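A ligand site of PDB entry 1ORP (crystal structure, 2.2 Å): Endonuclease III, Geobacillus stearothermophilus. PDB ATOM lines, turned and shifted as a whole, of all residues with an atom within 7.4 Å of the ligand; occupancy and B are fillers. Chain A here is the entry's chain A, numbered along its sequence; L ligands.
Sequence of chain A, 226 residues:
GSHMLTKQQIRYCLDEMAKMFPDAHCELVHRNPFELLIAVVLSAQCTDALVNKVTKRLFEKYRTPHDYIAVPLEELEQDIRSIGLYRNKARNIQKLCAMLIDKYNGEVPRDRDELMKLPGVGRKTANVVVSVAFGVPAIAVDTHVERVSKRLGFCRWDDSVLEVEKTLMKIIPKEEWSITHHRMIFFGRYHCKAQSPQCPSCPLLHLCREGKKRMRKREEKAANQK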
ATOM      1  N   CYS A  13      -5.154  11.207 -12.095  1.00  0.00           N
ATOM      2  CA  CYS A  13      -5.931  11.672 -10.959  1.00  0.00           C
ATOM      3  C   CYS A  13      -5.020  12.003  -9.774  1.00  0.00           C
ATOM      4  O   CYS A  13      -5.199  13.023  -9.102  1.00  0.00           O
ATOM      5  CB  CYS A  13      -6.923  10.595 -10.508  1.00  0.00           C
ATOM      6  SG  CYS A  13      -8.391  10.393 -11.518  1.00  0.00           S
ATOM      7  N   ARG A 147     -13.127   6.013   0.110  1.00  0.00           N
ATOM      8  CA  ARG A 147     -14.180   6.759  -0.577  1.00  0.00           C
ATOM      9  C   ARG A 147     -13.689   7.348  -1.888  1.00  0.00           C
ATOM     10  O   ARG A 147     -14.332   7.220  -2.931  1.00  0.00           O
ATOM     11  CB  ARG A 147     -14.694   7.894   0.337  1.00  0.00           C
ATOM     12  CG  ARG A 147     -15.877   8.663  -0.248  1.00  0.00           C
ATOM     13  CD  ARG A 147     -16.399   9.696   0.748  1.00  0.00           C
ATOM     14  NE  ARG A 147     -15.464  10.818   0.904  1.00  0.00           N
ATOM     15  CZ  ARG A 147     -14.804  11.095   2.029  1.00  0.00           C
ATOM     16  NH1 ARG A 147     -14.982  10.332   3.103  1.00  0.00           N
ATOM     17  NH2 ARG A 147     -13.963  12.117   2.064  1.00  0.00           N
ATOM     18  N   VAL A 148     -12.542   8.010  -1.827  1.00  0.00           N
ATOM     19  CA  VAL A 148     -11.983   8.646  -3.000  1.00  0.00           C
ATOM     20  C   VAL A 148     -11.668   7.623  -4.081  1.00  0.00           C
ATOM     21  O   VAL A 148     -11.973   7.859  -5.252  1.00  0.00           O
ATOM     22  CB  VAL A 148     -10.723   9.439  -2.639  1.00  0.00           C
ATOM     23  CG1 VAL A 148     -10.009   9.909  -3.892  1.00  0.00           C
ATOM     24  CG2 VAL A 148     -11.109  10.639  -1.786  1.00  0.00           C
ATOM     25  N   ARG A 151     -15.150   6.451  -5.403  1.00  0.00           N
ATOM     26  CA  ARG A 151     -15.866   7.471  -6.170  1.00  0.00           C
ATOM     27  C   ARG A 151     -15.215   7.719  -7.522  1.00  0.00           C
ATOM     28  O   ARG A 151     -15.887   7.878  -8.541  1.00  0.00           O
ATOM     29  CB  ARG A 151     -15.954   8.793  -5.403  1.00  0.00           C
ATOM     30  CG  ARG A 151     -16.961   8.789  -4.281  1.00  0.00           C
ATOM     31  CD  ARG A 151     -17.132  10.199  -3.723  1.00  0.00           C
ATOM     32  NE  ARG A 151     -18.079  10.235  -2.612  1.00  0.00           N
ATOM     33  CZ  ARG A 151     -18.188  11.256  -1.774  1.00  0.00           C
ATOM     34  NH1 ARG A 151     -17.417  12.327  -1.911  1.00  0.00           N
ATOM     35  NH2 ARG A 151     -19.054  11.203  -0.771  1.00  0.00           N
ATOM     36  N   LEU A 152     -13.889   7.745  -7.536  1.00  0.00           N
ATOM     37  CA  LEU A 152     -13.148   8.007  -8.762  1.00  0.00           C
ATOM     38  C   LEU A 152     -13.050   6.794  -9.677  1.00  0.00           C
ATOM     39  O   LEU A 152     -12.621   6.906 -10.825  1.00  0.00           O
ATOM     40  CB  LEU A 152     -11.743   8.490  -8.412  1.00  0.00           C
ATOM     41  CG  LEU A 152     -11.272   9.864  -8.887  1.00  0.00           C
ATOM     42  CD1 LEU A 152     -12.428  10.839  -8.933  1.00  0.00           C
ATOM     43  CD2 LEU A 152     -10.177  10.348  -7.955  1.00  0.00           C
ATOM     44  N   PHE A 187      -7.307  15.278  -0.225  1.00  0.00           N
ATOM     45  CA  PHE A 187      -8.283  15.373  -1.303  1.00  0.00           C
ATOM     46  C   PHE A 187      -9.670  15.013  -0.810  1.00  0.00           C
ATOM     47  O   PHE A 187     -10.646  15.689  -1.132  1.00  0.00           O
ATOM     48  CB  PHE A 187      -7.923  14.448  -2.472  1.00  0.00           C
ATOM     49  CG  PHE A 187      -8.866  14.571  -3.650  1.00  0.00           C
ATOM     50  CD1 PHE A 187      -8.721  15.616  -4.579  1.00  0.00           C
ATOM     51  CD2 PHE A 187      -9.926  13.671  -3.822  1.00  0.00           C
ATOM     52  CE1 PHE A 187      -9.618  15.758  -5.643  1.00  0.00           C
ATOM     53  CE2 PHE A 187     -10.819  13.812  -4.877  1.00  0.00           C
ATOM     54  CZ  PHE A 187     -10.666  14.855  -5.788  1.00  0.00           C
ATOM     55  N   GLY A 188      -9.758  13.957  -0.005  1.00  0.00           N
ATOM     56  CA  GLY A 188     -11.045  13.509   0.503  1.00  0.00           C
ATOM     57  C   GLY A 188     -11.545  14.279   1.698  1.00  0.00           C
ATOM     58  O   GLY A 188     -12.763  14.365   1.924  1.00  0.00           O
ATOM     59  N   HIS A 191     -11.918  18.197  -0.076  1.00  0.00           N
ATOM     60  CA  HIS A 191     -12.537  18.342  -1.392  1.00  0.00           C
ATOM     61  C   HIS A 191     -13.635  17.307  -1.657  1.00  0.00           C
ATOM     62  O   HIS A 191     -14.829  17.637  -1.618  1.00  0.00           O
ATOM     63  CB  HIS A 191     -11.458  18.239  -2.466  1.00  0.00           C
ATOM     64  CG  HIS A 191     -11.909  18.671  -3.820  1.00  0.00           C
ATOM     65  ND1 HIS A 191     -12.132  19.988  -4.142  1.00  0.00           N
ATOM     66  CD2 HIS A 191     -12.192  17.961  -4.935  1.00  0.00           C
ATOM     67  CE1 HIS A 191     -12.531  20.070  -5.394  1.00  0.00           C
ATOM     68  NE2 HIS A 191     -12.576  18.853  -5.899  1.00  0.00           N
ATOM     69  N   CYS A 192     -13.239  16.066  -1.927  1.00  0.00           N
ATOM     70  CA  CYS A 192     -14.214  15.002  -2.182  1.00  0.00           C
ATOM     71  C   CYS A 192     -14.802  14.518  -0.853  1.00  0.00           C
ATOM     72  O   CYS A 192     -14.747  13.326  -0.547  1.00  0.00           O
ATOM     73  CB  CYS A 192     -13.560  13.828  -2.919  1.00  0.00           C
ATOM     74  SG  CYS A 192     -14.684  12.461  -3.352  1.00  0.00           S
ATOM     75  N   LYS A 193     -15.341  15.454  -0.087  1.00  0.00           N
ATOM     76  CA  LYS A 193     -15.927  15.138   1.200  1.00  0.00           C
ATOM     77  C   LYS A 193     -17.013  14.090   1.125  1.00  0.00           C
ATOM     78  O   LYS A 193     -17.523  13.811   0.045  1.00  0.00           O
ATOM     79  N   SER A 196     -20.782  16.619   1.447  1.00  0.00           N
ATOM     80  CA  SER A 196     -20.917  17.459   0.274  1.00  0.00           C
ATOM     81  C   SER A 196     -19.661  17.640  -0.559  1.00  0.00           C
ATOM     82  O   SER A 196     -18.875  18.556  -0.301  1.00  0.00           O
ATOM     83  N   PRO A 197     -19.423  16.775  -1.562  1.00  0.00           N
ATOM     84  CA  PRO A 197     -18.227  16.897  -2.406  1.00  0.00           C
ATOM     85  C   PRO A 197     -18.264  18.127  -3.318  1.00  0.00           C
ATOM     86  O   PRO A 197     -19.321  18.506  -3.836  1.00  0.00           O
ATOM     87  CB  PRO A 197     -18.214  15.578  -3.184  1.00  0.00           C
ATOM     88  CG  PRO A 197     -19.670  15.227  -3.272  1.00  0.00           C
ATOM     89  CD  PRO A 197     -20.180  15.548  -1.891  1.00  0.00           C
ATOM     90  N   GLN A 198     -17.110  18.759  -3.503  1.00  0.00           N
ATOM     91  CA  GLN A 198     -16.992  19.941  -4.332  1.00  0.00           C
ATOM     92  C   GLN A 198     -16.797  19.595  -5.809  1.00  0.00           C
ATOM     93  O   GLN A 198     -15.877  20.084  -6.461  1.00  0.00           O
ATOM     94  CB  GLN A 198     -15.825  20.809  -3.860  1.00  0.00           C
ATOM     95  CG  GLN A 198     -15.873  21.172  -2.379  1.00  0.00           C
ATOM     96  CD  GLN A 198     -14.753  22.108  -1.979  1.00  0.00           C
ATOM     97  OE1 GLN A 198     -13.586  21.871  -2.294  1.00  0.00           O
ATOM     98  NE2 GLN A 198     -15.100  23.177  -1.274  1.00  0.00           N
ATOM     99  N   CYS A 199     -17.688  18.759  -6.333  1.00  0.00           N
ATOM    100  CA  CYS A 199     -17.602  18.325  -7.726  1.00  0.00           C
ATOM    101  C   CYS A 199     -17.587  19.491  -8.731  1.00  0.00           C
ATOM    102  O   CYS A 199     -16.669  19.586  -9.567  1.00  0.00           O
ATOM    103  CB  CYS A 199     -18.772  17.392  -8.061  1.00  0.00           C
ATOM    104  SG  CYS A 199     -19.213  16.263  -6.738  1.00  0.00           S
ATOM    105  N   PRO A 200     -18.586  20.386  -8.665  1.00  0.00           N
ATOM    106  CA  PRO A 200     -18.668  21.535  -9.575  1.00  0.00           C
ATOM    107  C   PRO A 200     -17.332  22.144  -9.960  1.00  0.00           C
ATOM    108  O   PRO A 200     -17.111  22.464 -11.122  1.00  0.00           O
ATOM    109  CB  PRO A 200     -19.557  22.511  -8.807  1.00  0.00           C
ATOM    110  CG  PRO A 200     -20.547  21.575  -8.149  1.00  0.00           C
ATOM    111  CD  PRO A 200     -19.641  20.460  -7.636  1.00  0.00           C
ATOM    112  N   SER A 201     -16.431  22.284  -8.994  1.00  0.00           N
ATOM    113  CA  SER A 201     -15.125  22.860  -9.293  1.00  0.00           C
ATOM    114  C   SER A 201     -13.983  21.866  -9.156  1.00  0.00           C
ATOM    115  O   SER A 201     -12.902  22.239  -8.708  1.00  0.00           O
ATOM    116  N   CYS A 202     -14.212  20.617  -9.539  1.00  0.00           N
ATOM    117  CA  CYS A 202     -13.192  19.582  -9.429  1.00  0.00           C
ATOM    118  C   CYS A 202     -12.498  19.261 -10.759  1.00  0.00           C
ATOM    119  O   CYS A 202     -13.143  19.087 -11.784  1.00  0.00           O
ATOM    120  CB  CYS A 202     -13.807  18.309  -8.851  1.00  0.00           C
ATOM    121  SG  CYS A 202     -12.628  16.955  -8.595  1.00  0.00           S
ATOM    122  N   PRO A 203     -11.158  19.183 -10.732  1.00  0.00           N
ATOM    123  CA  PRO A 203     -10.332  18.875 -11.910  1.00  0.00           C
ATOM    124  C   PRO A 203     -10.389  17.410 -12.309  1.00  0.00           C
ATOM    125  O   PRO A 203      -9.582  16.962 -13.130  1.00  0.00           O
ATOM    126  CB  PRO A 203      -8.922  19.276 -11.460  1.00  0.00           C
ATOM    127  CG  PRO A 203      -9.162  20.210 -10.298  1.00  0.00           C
ATOM    128  CD  PRO A 203     -10.315  19.565  -9.601  1.00  0.00           C
ATOM    129  N   LEU A 204     -11.314  16.664 -11.719  1.00  0.00           N
ATOM    130  CA  LEU A 204     -11.429  15.243 -12.024  1.00  0.00           C
ATOM    131  C   LEU A 204     -12.811  14.834 -12.519  1.00  0.00           C
ATOM    132  O   LEU A 204     -12.983  13.720 -13.004  1.00  0.00           O
ATOM    133  CB  LEU A 204     -11.039  14.400 -10.796  1.00  0.00           C
ATOM    134  CG  LEU A 204      -9.575  14.472 -10.362  1.00  0.00           C
ATOM    135  CD1 LEU A 204      -9.348  13.506  -9.206  1.00  0.00           C
ATOM    136  CD2 LEU A 204      -8.651  14.119 -11.521  1.00  0.00           C
ATOM    137  N   LEU A 205     -13.771  15.740 -12.393  1.00  0.00           N
ATOM    138  CA  LEU A 205     -15.140  15.462 -12.840  1.00  0.00           C
ATOM    139  C   LEU A 205     -15.181  14.969 -14.293  1.00  0.00           C
ATOM    140  O   LEU A 205     -16.025  14.139 -14.651  1.00  0.00           O
ATOM    141  CB  LEU A 205     -16.008  16.706 -12.683  1.00  0.00           C
ATOM    142  N   HIS A 206     -14.258  15.449 -15.122  1.00  0.00           N
ATOM    143  CA  HIS A 206     -14.217  15.071 -16.535  1.00  0.00           C
ATOM    144  C   HIS A 206     -13.909  13.599 -16.765  1.00  0.00           C
ATOM    145  O   HIS A 206     -13.971  13.113 -17.901  1.00  0.00           O
ATOM    146  CB  HIS A 206     -13.200  15.921 -17.298  1.00  0.00           C
ATOM    147  CG  HIS A 206     -11.791  15.500 -17.088  1.00  0.00           C
ATOM    148  ND1 HIS A 206     -11.086  15.777 -15.929  1.00  0.00           N
ATOM    149  CD2 HIS A 206     -10.928  14.842 -17.907  1.00  0.00           C
ATOM    150  CE1 HIS A 206      -9.856  15.309 -16.049  1.00  0.00           C
ATOM    151  NE2 HIS A 206      -9.734  14.734 -17.229  1.00  0.00           N
ATOM    152  N   LEU A 207     -13.559  12.886 -15.706  1.00  0.00           N
ATOM    153  CA  LEU A 207     -13.270  11.462 -15.803  1.00  0.00           C
ATOM    154  C   LEU A 207     -13.782  10.743 -14.559  1.00  0.00           C
ATOM    155  O   LEU A 207     -13.456   9.578 -14.335  1.00  0.00           O
ATOM    156  CB  LEU A 207     -11.772  11.210 -15.978  1.00  0.00           C
ATOM    157  CG  LEU A 207     -10.739  11.825 -15.031  1.00  0.00           C
ATOM    158  CD1 LEU A 207     -11.083  11.530 -13.585  1.00  0.00           C
ATOM    159  CD2 LEU A 207      -9.366  11.263 -15.385  1.00  0.00           C
ATOM    160  N   CYS A 208     -14.592  11.430 -13.772  1.00  0.00           N
ATOM    161  CA  CYS A 208     -15.123  10.848 -12.553  1.00  0.00           C
ATOM    162  C   CYS A 208     -16.561  10.373 -12.669  1.00  0.00           C
ATOM    163  O   CYS A 208     -17.447  11.150 -13.022  1.00  0.00           O
ATOM    164  CB  CYS A 208     -15.018  11.857 -11.414  1.00  0.00           C
ATOM    165  SG  CYS A 208     -15.645  11.198  -9.875  1.00  0.00           S
ATOM    166  N   ARG A 209     -16.794   9.097 -12.355  1.00  0.00           N
ATOM    167  CA  ARG A 209     -18.124   8.532 -12.438  1.00  0.00           C
ATOM    168  C   ARG A 209     -19.091   9.059 -11.389  1.00  0.00           C
ATOM    169  O   ARG A 209     -20.243   9.358 -11.698  1.00  0.00           O
ATOM    170  N   GLU A 210     -18.619   9.162 -10.153  1.00  0.00           N
ATOM    171  CA  GLU A 210     -19.454   9.664  -9.054  1.00  0.00           C
ATOM    172  C   GLU A 210     -19.729  11.157  -9.252  1.00  0.00           C
ATOM    173  O   GLU A 210     -20.815  11.655  -8.930  1.00  0.00           O
ATOM    174  CB  GLU A 210     -18.742   9.451  -7.718  1.00  0.00           C
ATOM    175  CG  GLU A 210     -19.567   9.820  -6.503  1.00  0.00           C
ATOM    176  CD  GLU A 210     -20.719   8.862  -6.269  1.00  0.00           C
ATOM    177  OE1 GLU A 210     -21.543   9.114  -5.358  1.00  0.00           O
ATOM    178  OE2 GLU A 210     -20.808   7.844  -6.989  1.00  0.00           O
ATOM    179  N   GLY A 211     -18.731  11.859  -9.790  1.00  0.00           N
ATOM    180  CA  GLY A 211     -18.871  13.288 -10.030  1.00  0.00           C
ATOM    181  C   GLY A 211     -19.853  13.642 -11.129  1.00  0.00           C
ATOM    182  O   GLY A 211     -20.556  14.639 -11.029  1.00  0.00           O
ATOM    183  N   LYS A 212     -19.886  12.852 -12.204  1.00  0.00           N
ATOM    184  CA  LYS A 212     -20.812  13.123 -13.301  1.00  0.00           C
ATOM    185  C   LYS A 212     -22.233  12.797 -12.878  1.00  0.00           C
ATOM    186  O   LYS A 212     -23.183  13.493 -13.242  1.00  0.00           O
ATOM    187  CB  LYS A 212     -20.417  12.331 -14.551  1.00  0.00           C
ATOM    188  CG  LYS A 212     -19.142  12.852 -15.212  1.00  0.00           C
ATOM    189  CD  LYS A 212     -18.772  12.042 -16.452  1.00  0.00           C
ATOM    190  N   ARG A 214     -23.207  12.961  -9.879  1.00  0.00           N
ATOM    191  CA  ARG A 214     -23.522  13.964  -8.876  1.00  0.00           C
ATOM    192  C   ARG A 214     -24.084  15.216  -9.526  1.00  0.00           C
ATOM    193  O   ARG A 214     -25.059  15.797  -9.048  1.00  0.00           O
ATOM    194  N   MET A 215     -23.460  15.627 -10.625  1.00  0.00           N
ATOM    195  CA  MET A 215     -23.902  16.804 -11.356  1.00  0.00           C
ATOM    196  C   MET A 215     -25.242  16.515 -12.013  1.00  0.00           C
ATOM    197  O   MET A 215     -26.242  17.181 -11.735  1.00  0.00           O
ATOM    198  CB  MET A 215     -22.855  17.195 -12.409  1.00  0.00           C
ATOM    199  CG  MET A 215     -21.465  17.475 -11.839  1.00  0.00           C
ATOM    200  SD  MET A 215     -21.462  18.723 -10.529  1.00  0.00           S
ATOM    201  CE  MET A 215     -21.074  20.212 -11.461  1.00  0.00           C
HETATM  202 FE1  LIG L   1     -14.236  15.371  -7.799  1.00  0.00          FE
HETATM  203 FE2  LIG L   1     -14.984  13.688  -5.635  1.00  0.00          FE
HETATM  204 FE3  LIG L   1     -16.874  15.043  -7.190  1.00  0.00          FE
HETATM  205 FE4  LIG L   1     -15.468  12.931  -8.207  1.00  0.00          FE
HETATM  206  S1  LIG L   1     -17.069  12.900  -6.416  1.00  0.00           S
HETATM  207  S2  LIG L   1     -15.938  14.804  -9.131  1.00  0.00           S
HETATM  208  S3  LIG L   1     -13.482  13.211  -7.141  1.00  0.00           S
HETATM  209  S4  LIG L   1     -15.366  15.963  -5.877  1.00  0.00           S
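Arg 151 touches the ligand.
Leu 152 touches the ligand (CD1 to S3, 3.2 Å).
Phe 187 touches the ligand (CZ to S3, 3.5 Å).
CD2 of His 191 touches S4 of the ligand, at 3.9 Å.
Pro 197 touches the ligand (CB to S4, 3.9 Å).
Gln 198 touches the ligand.
Leu 205 touches the ligand.
Glu 210 touches the ligand (CG to S1, 3.97 Å).
CA of Gly 211 touches S2 of the ligand (3.4 Å).
13 residues have an atom within 4 Å of the ligand: Arg 151, Leu 152, Phe 187, His 191, Cys 192, Pro 197, Gln 198, Cys 199, Cys 202, Leu 205, Cys 208, Glu 210 and Gly 211.
The nearest printed residue that does not touch the ligand is Leu 204 (4.5 Å).
The backbone NH of Gly 211 sits close to the side-chain sulfur of Cys 208, at 3.2 Å.
The backbone carbonyl oxygen (O) of Cys 192 sits at hydrogen-bond distance from the guanidinium group (NH2) of Arg 147, 3.0 Å away.
The backbone carbonyl oxygen of Cys 192 is in hydrogen-bond range of the guanidinium group of Arg 151 (3.2 Å).
The backbone NH (N) of Glu 210 lies close to the backbone carbonyl oxygen (O) of Arg 151, 3.4 Å away.
The backbone NH (N) of Cys 192 is in hydrogen-bond range of the backbone carbonyl oxygen (O) of Phe 187, at 2.7 Å.
OE1 of Gln 198 is in hydrogen-bond range of ND1 of His 191, 3.0 Å away.
The side-chain sulfur (SG) of Cys 199 lies close to the backbone carbonyl oxygen (O) of Pro 197 (3.7 Å).
The side-chain sulfur of Cys 202 lies close to a ring nitrogen (NE2) of His 191 (3.3 Å).
The backbone NH of Cys 199 lies close to a sulfur (S4) of the ligand (3.7 Å).
The side-chain sulfur (SG) of Cys 192 is bound to an iron atom (FE2) of the ligand, 2.6 Å away.
An iron atom (FE1) of the ligand is bound by the side-chain sulfur (SG) of Cys 202, at 2.4 Å.
The side-chain sulfur (SG) of Cys 199 binds an iron atom (FE3) of the ligand.
An iron atom (FE4) of the ligand is bound by the side-chain sulfur (SG) of Cys 208 (2.4 Å).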
